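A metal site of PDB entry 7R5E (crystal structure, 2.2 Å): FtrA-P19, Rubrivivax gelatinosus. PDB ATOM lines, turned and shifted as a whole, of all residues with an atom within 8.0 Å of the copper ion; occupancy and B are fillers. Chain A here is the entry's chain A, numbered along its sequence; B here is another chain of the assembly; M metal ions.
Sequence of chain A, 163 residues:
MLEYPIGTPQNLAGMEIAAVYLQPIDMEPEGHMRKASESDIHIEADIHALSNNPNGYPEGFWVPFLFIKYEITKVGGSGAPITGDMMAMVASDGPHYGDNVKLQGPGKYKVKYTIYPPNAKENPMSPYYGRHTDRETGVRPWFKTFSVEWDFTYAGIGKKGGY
A ring nitrogen (ND1) of His 42 is in hydrogen-bond range of the backbone carbonyl oxygen (O) of Asp 99 (3.4 Å).
The backbone NH (N) of His 42 lies within hydrogen-bond range of the backbone carbonyl oxygen (O) of Leu 22 (2.9 Å).
The side-chain amide oxygen of Asn 100 is in hydrogen-bond range of a ring nitrogen (ND1) of His 42, at 2.8 Å.
A ring nitrogen (NE2) of His 96 sits close to the side-chain carboxylate (OE2) of Glu 44.
A ring nitrogen (ND1) of His 96 sits at hydrogen-bond distance from the backbone carbonyl oxygen (O) of Gly 94 (3.3 Å).
O of Val 90 lies within hydrogen-bond range of N of His 132 of chain B (2.9 Å).
ND1 of His 132 of chain B sits at hydrogen-bond distance from OG1 of Thr 137 of chain B, 2.7 Å away.
The copper ion is bound by NE2 of His 42, at 2.1 Å.
A ring nitrogen (NE2) of His 96 binds the copper ion, at 2.2 Å.
NE2 of His 132 of chain B is bound to the copper ion (2.2 Å).
SD of Met 89 binds the copper ion (2.4 Å).
The copper ion has four donor atoms within binding distance.
Glu 44 touches the copper ion (OE2 to CU, 3.9 Å).
Five residues have an atom within 4 Å of the copper ion: His 42, Glu 44, Met 89, His 96 and His 132 of chain B.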
ATOM      1  N   LEU A  22     -17.340  19.175  26.159  1.00  0.00           N
ATOM      2  CA  LEU A  22     -16.156  18.746  26.890  1.00  0.00           C
ATOM      3  C   LEU A  22     -14.987  19.016  25.961  1.00  0.00           C
ATOM      4  O   LEU A  22     -15.175  19.683  24.930  1.00  0.00           O
ATOM      5  CB  LEU A  22     -16.276  17.245  27.289  1.00  0.00           C
ATOM      6  CG  LEU A  22     -16.453  16.232  26.138  1.00  0.00           C
ATOM      7  CD1 LEU A  22     -15.840  14.890  26.501  1.00  0.00           C
ATOM      8  CD2 LEU A  22     -17.888  16.046  25.743  1.00  0.00           C
ATOM      9  N   GLN A  23     -13.799  18.550  26.307  1.00  0.00           N
ATOM     10  CA  GLN A  23     -12.603  18.707  25.490  1.00  0.00           C
ATOM     11  C   GLN A  23     -12.785  18.017  24.105  1.00  0.00           C
ATOM     12  O   GLN A  23     -13.533  17.038  24.020  1.00  0.00           O
ATOM     13  CB  GLN A  23     -11.381  18.098  26.209  1.00  0.00           C
ATOM     14  CG  GLN A  23     -11.399  16.538  26.340  1.00  0.00           C
ATOM     15  CD  GLN A  23     -12.037  16.039  27.614  1.00  0.00           C
ATOM     16  OE1 GLN A  23     -12.839  16.729  28.257  1.00  0.00           O
ATOM     17  NE2 GLN A  23     -11.656  14.835  28.025  1.00  0.00           N
ATOM     18  N   ILE A  25     -12.211  15.366  21.230  1.00  0.00           N
ATOM     19  CA  ILE A  25     -11.872  13.951  21.383  1.00  0.00           C
ATOM     20  C   ILE A  25     -11.186  13.375  20.156  1.00  0.00           C
ATOM     21  O   ILE A  25     -11.062  14.052  19.140  1.00  0.00           O
ATOM     22  CB  ILE A  25     -13.142  13.154  21.781  1.00  0.00           C
ATOM     23  CG1 ILE A  25     -14.286  13.282  20.727  1.00  0.00           C
ATOM     24  CG2 ILE A  25     -13.624  13.504  23.176  1.00  0.00           C
ATOM     25  CD1 ILE A  25     -14.278  12.253  19.520  1.00  0.00           C
ATOM     26  N   ASP A  26     -10.760  12.095  20.251  1.00  0.00           N
ATOM     27  CA  ASP A  26     -10.201  11.273  19.173  1.00  0.00           C
ATOM     28  C   ASP A  26     -11.219  10.156  18.926  1.00  0.00           C
ATOM     29  O   ASP A  26     -11.825   9.638  19.893  1.00  0.00           O
ATOM     30  CB  ASP A  26      -8.850  10.661  19.553  1.00  0.00           C
ATOM     31  CG  ASP A  26      -7.784  11.647  19.998  1.00  0.00           C
ATOM     32  OD1 ASP A  26      -7.807  12.817  19.526  1.00  0.00           O
ATOM     33  OD2 ASP A  26      -6.922  11.258  20.818  1.00  0.00           O
ATOM     34  N   MET A  27     -11.439   9.826  17.653  1.00  0.00           N
ATOM     35  CA  MET A  27     -12.451   8.864  17.268  1.00  0.00           C
ATOM     36  C   MET A  27     -11.988   7.977  16.126  1.00  0.00           C
ATOM     37  O   MET A  27     -11.243   8.424  15.249  1.00  0.00           O
ATOM     38  CB  MET A  27     -13.706   9.660  16.823  1.00  0.00           C
ATOM     39  CG  MET A  27     -14.978   8.829  16.673  1.00  0.00           C
ATOM     40  SD  MET A  27     -16.213   9.664  15.631  1.00  0.00           S
ATOM     41  CE  MET A  27     -15.624   9.159  14.011  1.00  0.00           C
ATOM     42  N   MET A  33     -13.990  13.250  12.290  1.00  0.00           N
ATOM     43  CA  MET A  33     -13.969  14.377  13.211  1.00  0.00           C
ATOM     44  C   MET A  33     -12.883  15.311  12.774  1.00  0.00           C
ATOM     45  O   MET A  33     -11.817  14.873  12.359  1.00  0.00           O
ATOM     46  CB  MET A  33     -13.601  13.948  14.669  1.00  0.00           C
ATOM     47  CG  MET A  33     -14.634  13.126  15.385  1.00  0.00           C
ATOM     48  SD  MET A  33     -16.040  14.094  15.909  1.00  0.00           S
ATOM     49  CE  MET A  33     -17.253  13.587  14.628  1.00  0.00           C
ATOM     50  N   HIS A  42     -15.759  19.338  22.125  1.00  0.00           N
ATOM     51  CA  HIS A  42     -16.534  18.261  21.570  1.00  0.00           C
ATOM     52  C   HIS A  42     -17.955  18.607  22.014  1.00  0.00           C
ATOM     53  O   HIS A  42     -18.193  18.723  23.213  1.00  0.00           O
ATOM     54  CB  HIS A  42     -16.129  16.893  22.095  1.00  0.00           C
ATOM     55  CG  HIS A  42     -16.797  15.773  21.359  1.00  0.00           C
ATOM     56  ND1 HIS A  42     -16.566  15.551  20.007  1.00  0.00           N
ATOM     57  CD2 HIS A  42     -17.647  14.834  21.819  1.00  0.00           C
ATOM     58  CE1 HIS A  42     -17.294  14.492  19.693  1.00  0.00           C
ATOM     59  NE2 HIS A  42     -17.955  14.029  20.753  1.00  0.00           N
ATOM     60  N   ILE A  43     -18.856  18.878  21.071  1.00  0.00           N
ATOM     61  CA  ILE A  43     -20.223  19.227  21.416  1.00  0.00           C
ATOM     62  C   ILE A  43     -21.096  17.965  21.296  1.00  0.00           C
ATOM     63  O   ILE A  43     -20.914  17.178  20.372  1.00  0.00           O
ATOM     64  CB  ILE A  43     -20.730  20.444  20.597  1.00  0.00           C
ATOM     65  CG1 ILE A  43     -21.984  21.045  21.261  1.00  0.00           C
ATOM     66  CG2 ILE A  43     -20.966  20.058  19.089  1.00  0.00           C
ATOM     67  CD1 ILE A  43     -22.399  22.434  20.817  1.00  0.00           C
ATOM     68  N   GLU A  44     -22.001  17.748  22.246  1.00  0.00           N
ATOM     69  CA  GLU A  44     -22.837  16.553  22.216  1.00  0.00           C
ATOM     70  C   GLU A  44     -24.321  16.845  22.346  1.00  0.00           C
ATOM     71  O   GLU A  44     -24.716  17.868  22.899  1.00  0.00           O
ATOM     72  CB  GLU A  44     -22.448  15.577  23.325  1.00  0.00           C
ATOM     73  CG  GLU A  44     -21.003  15.077  23.278  1.00  0.00           C
ATOM     74  CD  GLU A  44     -20.604  14.091  24.370  1.00  0.00           C
ATOM     75  OE1 GLU A  44     -21.378  13.904  25.326  1.00  0.00           O
ATOM     76  OE2 GLU A  44     -19.499  13.513  24.247  1.00  0.00           O
ATOM     77  N   ALA A  45     -25.126  15.938  21.786  1.00  0.00           N
ATOM     78  CA  ALA A  45     -26.570  15.913  21.942  1.00  0.00           C
ATOM     79  C   ALA A  45     -26.821  14.591  22.656  1.00  0.00           C
ATOM     80  O   ALA A  45     -26.413  13.531  22.167  1.00  0.00           O
ATOM     81  CB  ALA A  45     -27.278  15.955  20.596  1.00  0.00           C
ATOM     82  N   MET A  87     -22.314  13.265  14.524  1.00  0.00           N
ATOM     83  CA  MET A  87     -22.186  11.888  14.133  1.00  0.00           C
ATOM     84  C   MET A  87     -22.506  11.037  15.368  1.00  0.00           C
ATOM     85  O   MET A  87     -22.167  11.454  16.473  1.00  0.00           O
ATOM     86  CB  MET A  87     -20.752  11.655  13.645  1.00  0.00           C
ATOM     87  CG  MET A  87     -20.556  10.325  13.036  1.00  0.00           C
ATOM     88  SD  MET A  87     -18.863  10.080  12.570  1.00  0.00           S
ATOM     89  CE  MET A  87     -18.945   8.297  12.115  1.00  0.00           C
ATOM     90  N   ALA A  88     -23.191   9.891  15.194  1.00  0.00           N
ATOM     91  CA  ALA A  88     -23.481   8.930  16.257  1.00  0.00           C
ATOM     92  C   ALA A  88     -22.162   8.237  16.594  1.00  0.00           C
ATOM     93  O   ALA A  88     -21.368   7.966  15.708  1.00  0.00           O
ATOM     94  CB  ALA A  88     -24.494   7.877  15.789  1.00  0.00           C
ATOM     95  N   MET A  89     -21.906   8.015  17.876  1.00  0.00           N
ATOM     96  CA  MET A  89     -20.675   7.403  18.369  1.00  0.00           C
ATOM     97  C   MET A  89     -20.852   6.923  19.797  1.00  0.00           C
ATOM     98  O   MET A  89     -21.829   7.250  20.438  1.00  0.00           O
ATOM     99  CB  MET A  89     -19.476   8.371  18.286  1.00  0.00           C
ATOM    100  CG  MET A  89     -19.658   9.615  19.082  1.00  0.00           C
ATOM    101  SD  MET A  89     -18.391  10.848  18.746  1.00  0.00           S
ATOM    102  CE  MET A  89     -18.966  11.569  17.291  1.00  0.00           C
ATOM    103  N   VAL A  90     -19.888   6.157  20.290  1.00  0.00           N
ATOM    104  CA  VAL A  90     -19.889   5.671  21.662  1.00  0.00           C
ATOM    105  C   VAL A  90     -18.616   6.126  22.366  1.00  0.00           C
ATOM    106  O   VAL A  90     -17.539   6.206  21.763  1.00  0.00           O
ATOM    107  CB  VAL A  90     -20.139   4.151  21.747  1.00  0.00           C
ATOM    108  CG1 VAL A  90     -18.913   3.353  21.327  1.00  0.00           C
ATOM    109  CG2 VAL A  90     -20.619   3.738  23.158  1.00  0.00           C
ATOM    110  N   ALA A  91     -18.771   6.463  23.637  1.00  0.00           N
ATOM    111  CA  ALA A  91     -17.724   6.914  24.538  1.00  0.00           C
ATOM    112  C   ALA A  91     -17.948   6.158  25.877  1.00  0.00           C
ATOM    113  O   ALA A  91     -18.861   5.324  25.961  1.00  0.00           O
ATOM    114  CB  ALA A  91     -17.806   8.424  24.717  1.00  0.00           C
ATOM    115  N   ASP A  93     -19.186   6.978  28.672  1.00  0.00           N
ATOM    116  CA  ASP A  93     -20.490   7.261  29.277  1.00  0.00           C
ATOM    117  C   ASP A  93     -21.687   6.801  28.404  1.00  0.00           C
ATOM    118  O   ASP A  93     -22.844   7.049  28.757  1.00  0.00           O
ATOM    119  CB  ASP A  93     -20.589   8.775  29.635  1.00  0.00           C
ATOM    120  CG  ASP A  93     -20.601   9.755  28.457  1.00  0.00           C
ATOM    121  OD1 ASP A  93     -20.204   9.350  27.326  1.00  0.00           O
ATOM    122  OD2 ASP A  93     -21.003  10.929  28.672  1.00  0.00           O
ATOM    123  N   GLY A  94     -21.408   6.149  27.282  1.00  0.00           N
ATOM    124  CA  GLY A  94     -22.423   5.580  26.401  1.00  0.00           C
ATOM    125  C   GLY A  94     -22.502   6.206  25.039  1.00  0.00           C
ATOM    126  O   GLY A  94     -21.729   7.120  24.709  1.00  0.00           O
ATOM    127  N   PRO A  95     -23.499   5.774  24.229  1.00  0.00           N
ATOM    128  CA  PRO A  95     -23.654   6.355  22.888  1.00  0.00           C
ATOM    129  C   PRO A  95     -24.299   7.736  22.923  1.00  0.00           C
ATOM    130  O   PRO A  95     -25.062   8.058  23.830  1.00  0.00           O
ATOM    131  CB  PRO A  95     -24.527   5.321  22.155  1.00  0.00           C
ATOM    132  CG  PRO A  95     -25.316   4.701  23.211  1.00  0.00           C
ATOM    133  CD  PRO A  95     -24.526   4.729  24.483  1.00  0.00           C
ATOM    134  N   HIS A  96     -23.944   8.543  21.955  1.00  0.00           N
ATOM    135  CA  HIS A  96     -24.423   9.909  21.825  1.00  0.00           C
ATOM    136  C   HIS A  96     -24.183  10.392  20.377  1.00  0.00           C
ATOM    137  O   HIS A  96     -23.691   9.634  19.542  1.00  0.00           O
ATOM    138  CB  HIS A  96     -23.711  10.815  22.871  1.00  0.00           C
ATOM    139  CG  HIS A  96     -22.237  10.910  22.627  1.00  0.00           C
ATOM    140  ND1 HIS A  96     -21.364   9.924  23.071  1.00  0.00           N
ATOM    141  CD2 HIS A  96     -21.535  11.822  21.917  1.00  0.00           C
ATOM    142  CE1 HIS A  96     -20.168  10.301  22.658  1.00  0.00           C
ATOM    143  NE2 HIS A  96     -20.214  11.448  21.979  1.00  0.00           N
ATOM    144  N   TYR A  97     -24.518  11.662  20.101  1.00  0.00           N
ATOM    145  CA  TYR A  97     -24.299  12.364  18.845  1.00  0.00           C
ATOM    146  C   TYR A  97     -23.337  13.485  19.203  1.00  0.00           C
ATOM    147  O   TYR A  97     -23.565  14.177  20.171  1.00  0.00           O
ATOM    148  CB  TYR A  97     -25.621  12.925  18.269  1.00  0.00           C
ATOM    149  CG  TYR A  97     -26.633  11.843  18.015  1.00  0.00           C
ATOM    150  CD1 TYR A  97     -26.568  11.050  16.857  1.00  0.00           C
ATOM    151  CD2 TYR A  97     -27.628  11.547  18.946  1.00  0.00           C
ATOM    152  CE1 TYR A  97     -27.497  10.041  16.617  1.00  0.00           C
ATOM    153  CE2 TYR A  97     -28.549  10.536  18.717  1.00  0.00           C
ATOM    154  CZ  TYR A  97     -28.478   9.778  17.552  1.00  0.00           C
ATOM    155  OH  TYR A  97     -29.351   8.755  17.356  1.00  0.00           O
ATOM    156  N   GLY A  98     -22.213  13.571  18.488  1.00  0.00           N
ATOM    157  CA  GLY A  98     -21.206  14.568  18.802  1.00  0.00           C
ATOM    158  C   GLY A  98     -20.407  15.048  17.612  1.00  0.00           C
ATOM    159  O   GLY A  98     -20.500  14.477  16.515  1.00  0.00           O
ATOM    160  N   ASP A  99     -19.629  16.127  17.831  1.00  0.00           N
ATOM    161  CA  ASP A  99     -18.716  16.700  16.837  1.00  0.00           C
ATOM    162  C   ASP A  99     -17.623  17.524  17.483  1.00  0.00           C
ATOM    163  O   ASP A  99     -17.898  18.229  18.453  1.00  0.00           O
ATOM    164  CB  ASP A  99     -19.482  17.592  15.827  1.00  0.00           C
ATOM    165  CG  ASP A  99     -18.818  17.669  14.466  1.00  0.00           C
ATOM    166  OD1 ASP A  99     -18.000  16.767  14.146  1.00  0.00           O
ATOM    167  OD2 ASP A  99     -19.074  18.637  13.735  1.00  0.00           O
ATOM    168  N   ASN A 100     -16.391  17.518  16.878  1.00  0.00           N
ATOM    169  CA  ASN A 100     -15.340  18.400  17.362  1.00  0.00           C
ATOM    170  C   ASN A 100     -15.589  19.734  16.683  1.00  0.00           C
ATOM    171  O   ASN A 100     -15.887  19.765  15.489  1.00  0.00           O
ATOM    172  CB  ASN A 100     -13.887  17.878  17.147  1.00  0.00           C
ATOM    173  CG  ASN A 100     -13.429  16.781  18.091  1.00  0.00           C
ATOM    174  OD1 ASN A 100     -14.042  16.495  19.127  1.00  0.00           O
ATOM    175  ND2 ASN A 100     -12.334  16.133  17.745  1.00  0.00           N
ATOM    176  N   GLY B 130     -19.133   5.979  15.162  1.00  0.00           N
ATOM    177  CA  GLY B 130     -17.791   6.144  15.681  1.00  0.00           C
ATOM    178  C   GLY B 130     -17.596   5.554  17.062  1.00  0.00           C
ATOM    179  O   GLY B 130     -18.517   5.021  17.692  1.00  0.00           O
ATOM    180  N   ARG B 131     -16.382   5.702  17.557  1.00  0.00           N
ATOM    181  CA  ARG B 131     -15.950   5.196  18.825  1.00  0.00           C
ATOM    182  C   ARG B 131     -14.842   6.144  19.340  1.00  0.00           C
ATOM    183  O   ARG B 131     -13.857   6.341  18.638  1.00  0.00           O
ATOM    184  CB  ARG B 131     -15.405   3.755  18.580  1.00  0.00           C
ATOM    185  CG  ARG B 131     -14.730   3.143  19.735  1.00  0.00           C
ATOM    186  CD  ARG B 131     -14.282   1.735  19.469  1.00  0.00           C
ATOM    187  NE  ARG B 131     -13.039   1.690  18.709  1.00  0.00           N
ATOM    188  CZ  ARG B 131     -11.817   1.815  19.238  1.00  0.00           C
ATOM    189  NH1 ARG B 131     -11.665   2.019  20.540  1.00  0.00           N
ATOM    190  NH2 ARG B 131     -10.741   1.735  18.461  1.00  0.00           N
ATOM    191  N   HIS B 132     -14.987   6.719  20.564  1.00  0.00           N
ATOM    192  CA  HIS B 132     -13.912   7.525  21.159  1.00  0.00           C
ATOM    193  C   HIS B 132     -12.743   6.623  21.483  1.00  0.00           C
ATOM    194  O   HIS B 132     -12.942   5.483  21.908  1.00  0.00           O
ATOM    195  CB  HIS B 132     -14.348   8.241  22.457  1.00  0.00           C
ATOM    196  CG  HIS B 132     -15.285   9.393  22.270  1.00  0.00           C
ATOM    197  ND1 HIS B 132     -15.344  10.410  23.178  1.00  0.00           N
ATOM    198  CD2 HIS B 132     -16.218   9.621  21.317  1.00  0.00           C
ATOM    199  CE1 HIS B 132     -16.331  11.194  22.801  1.00  0.00           C
ATOM    200  NE2 HIS B 132     -16.829  10.797  21.647  1.00  0.00           N
ATOM    201  N   ASP B 134      -9.631   8.353  22.852  1.00  0.00           N
ATOM    202  CA  ASP B 134      -8.764   9.103  23.807  1.00  0.00           C
ATOM    203  C   ASP B 134      -8.795   8.459  25.219  1.00  0.00           C
ATOM    204  O   ASP B 134      -9.717   7.716  25.508  1.00  0.00           O
ATOM    205  CB  ASP B 134      -9.173  10.589  23.856  1.00  0.00           C
ATOM    206  CG  ASP B 134     -10.658  10.762  24.117  1.00  0.00           C
ATOM    207  OD1 ASP B 134     -11.452  10.571  23.173  1.00  0.00           O
ATOM    208  OD2 ASP B 134     -11.018  11.035  25.297  1.00  0.00           O
ATOM    209  N   THR B 137     -12.150   9.530  27.688  1.00  0.00           N
ATOM    210  CA  THR B 137     -13.528   9.152  27.291  1.00  0.00           C
ATOM    211  C   THR B 137     -13.592   7.962  26.356  1.00  0.00           C
ATOM    212  O   THR B 137     -14.692   7.559  25.958  1.00  0.00           O
ATOM    213  CB  THR B 137     -14.258  10.377  26.651  1.00  0.00           C
ATOM    214  OG1 THR B 137     -13.732  10.627  25.347  1.00  0.00           O
ATOM    215  CG2 THR B 137     -14.177  11.633  27.515  1.00  0.00           C
HETATM  216 CU    CU M   1     -18.477  11.980  20.808  1.00  0.00          CU
HETATM  217 MG    MG M   2     -21.688  12.507  27.582  1.00  0.00          MG
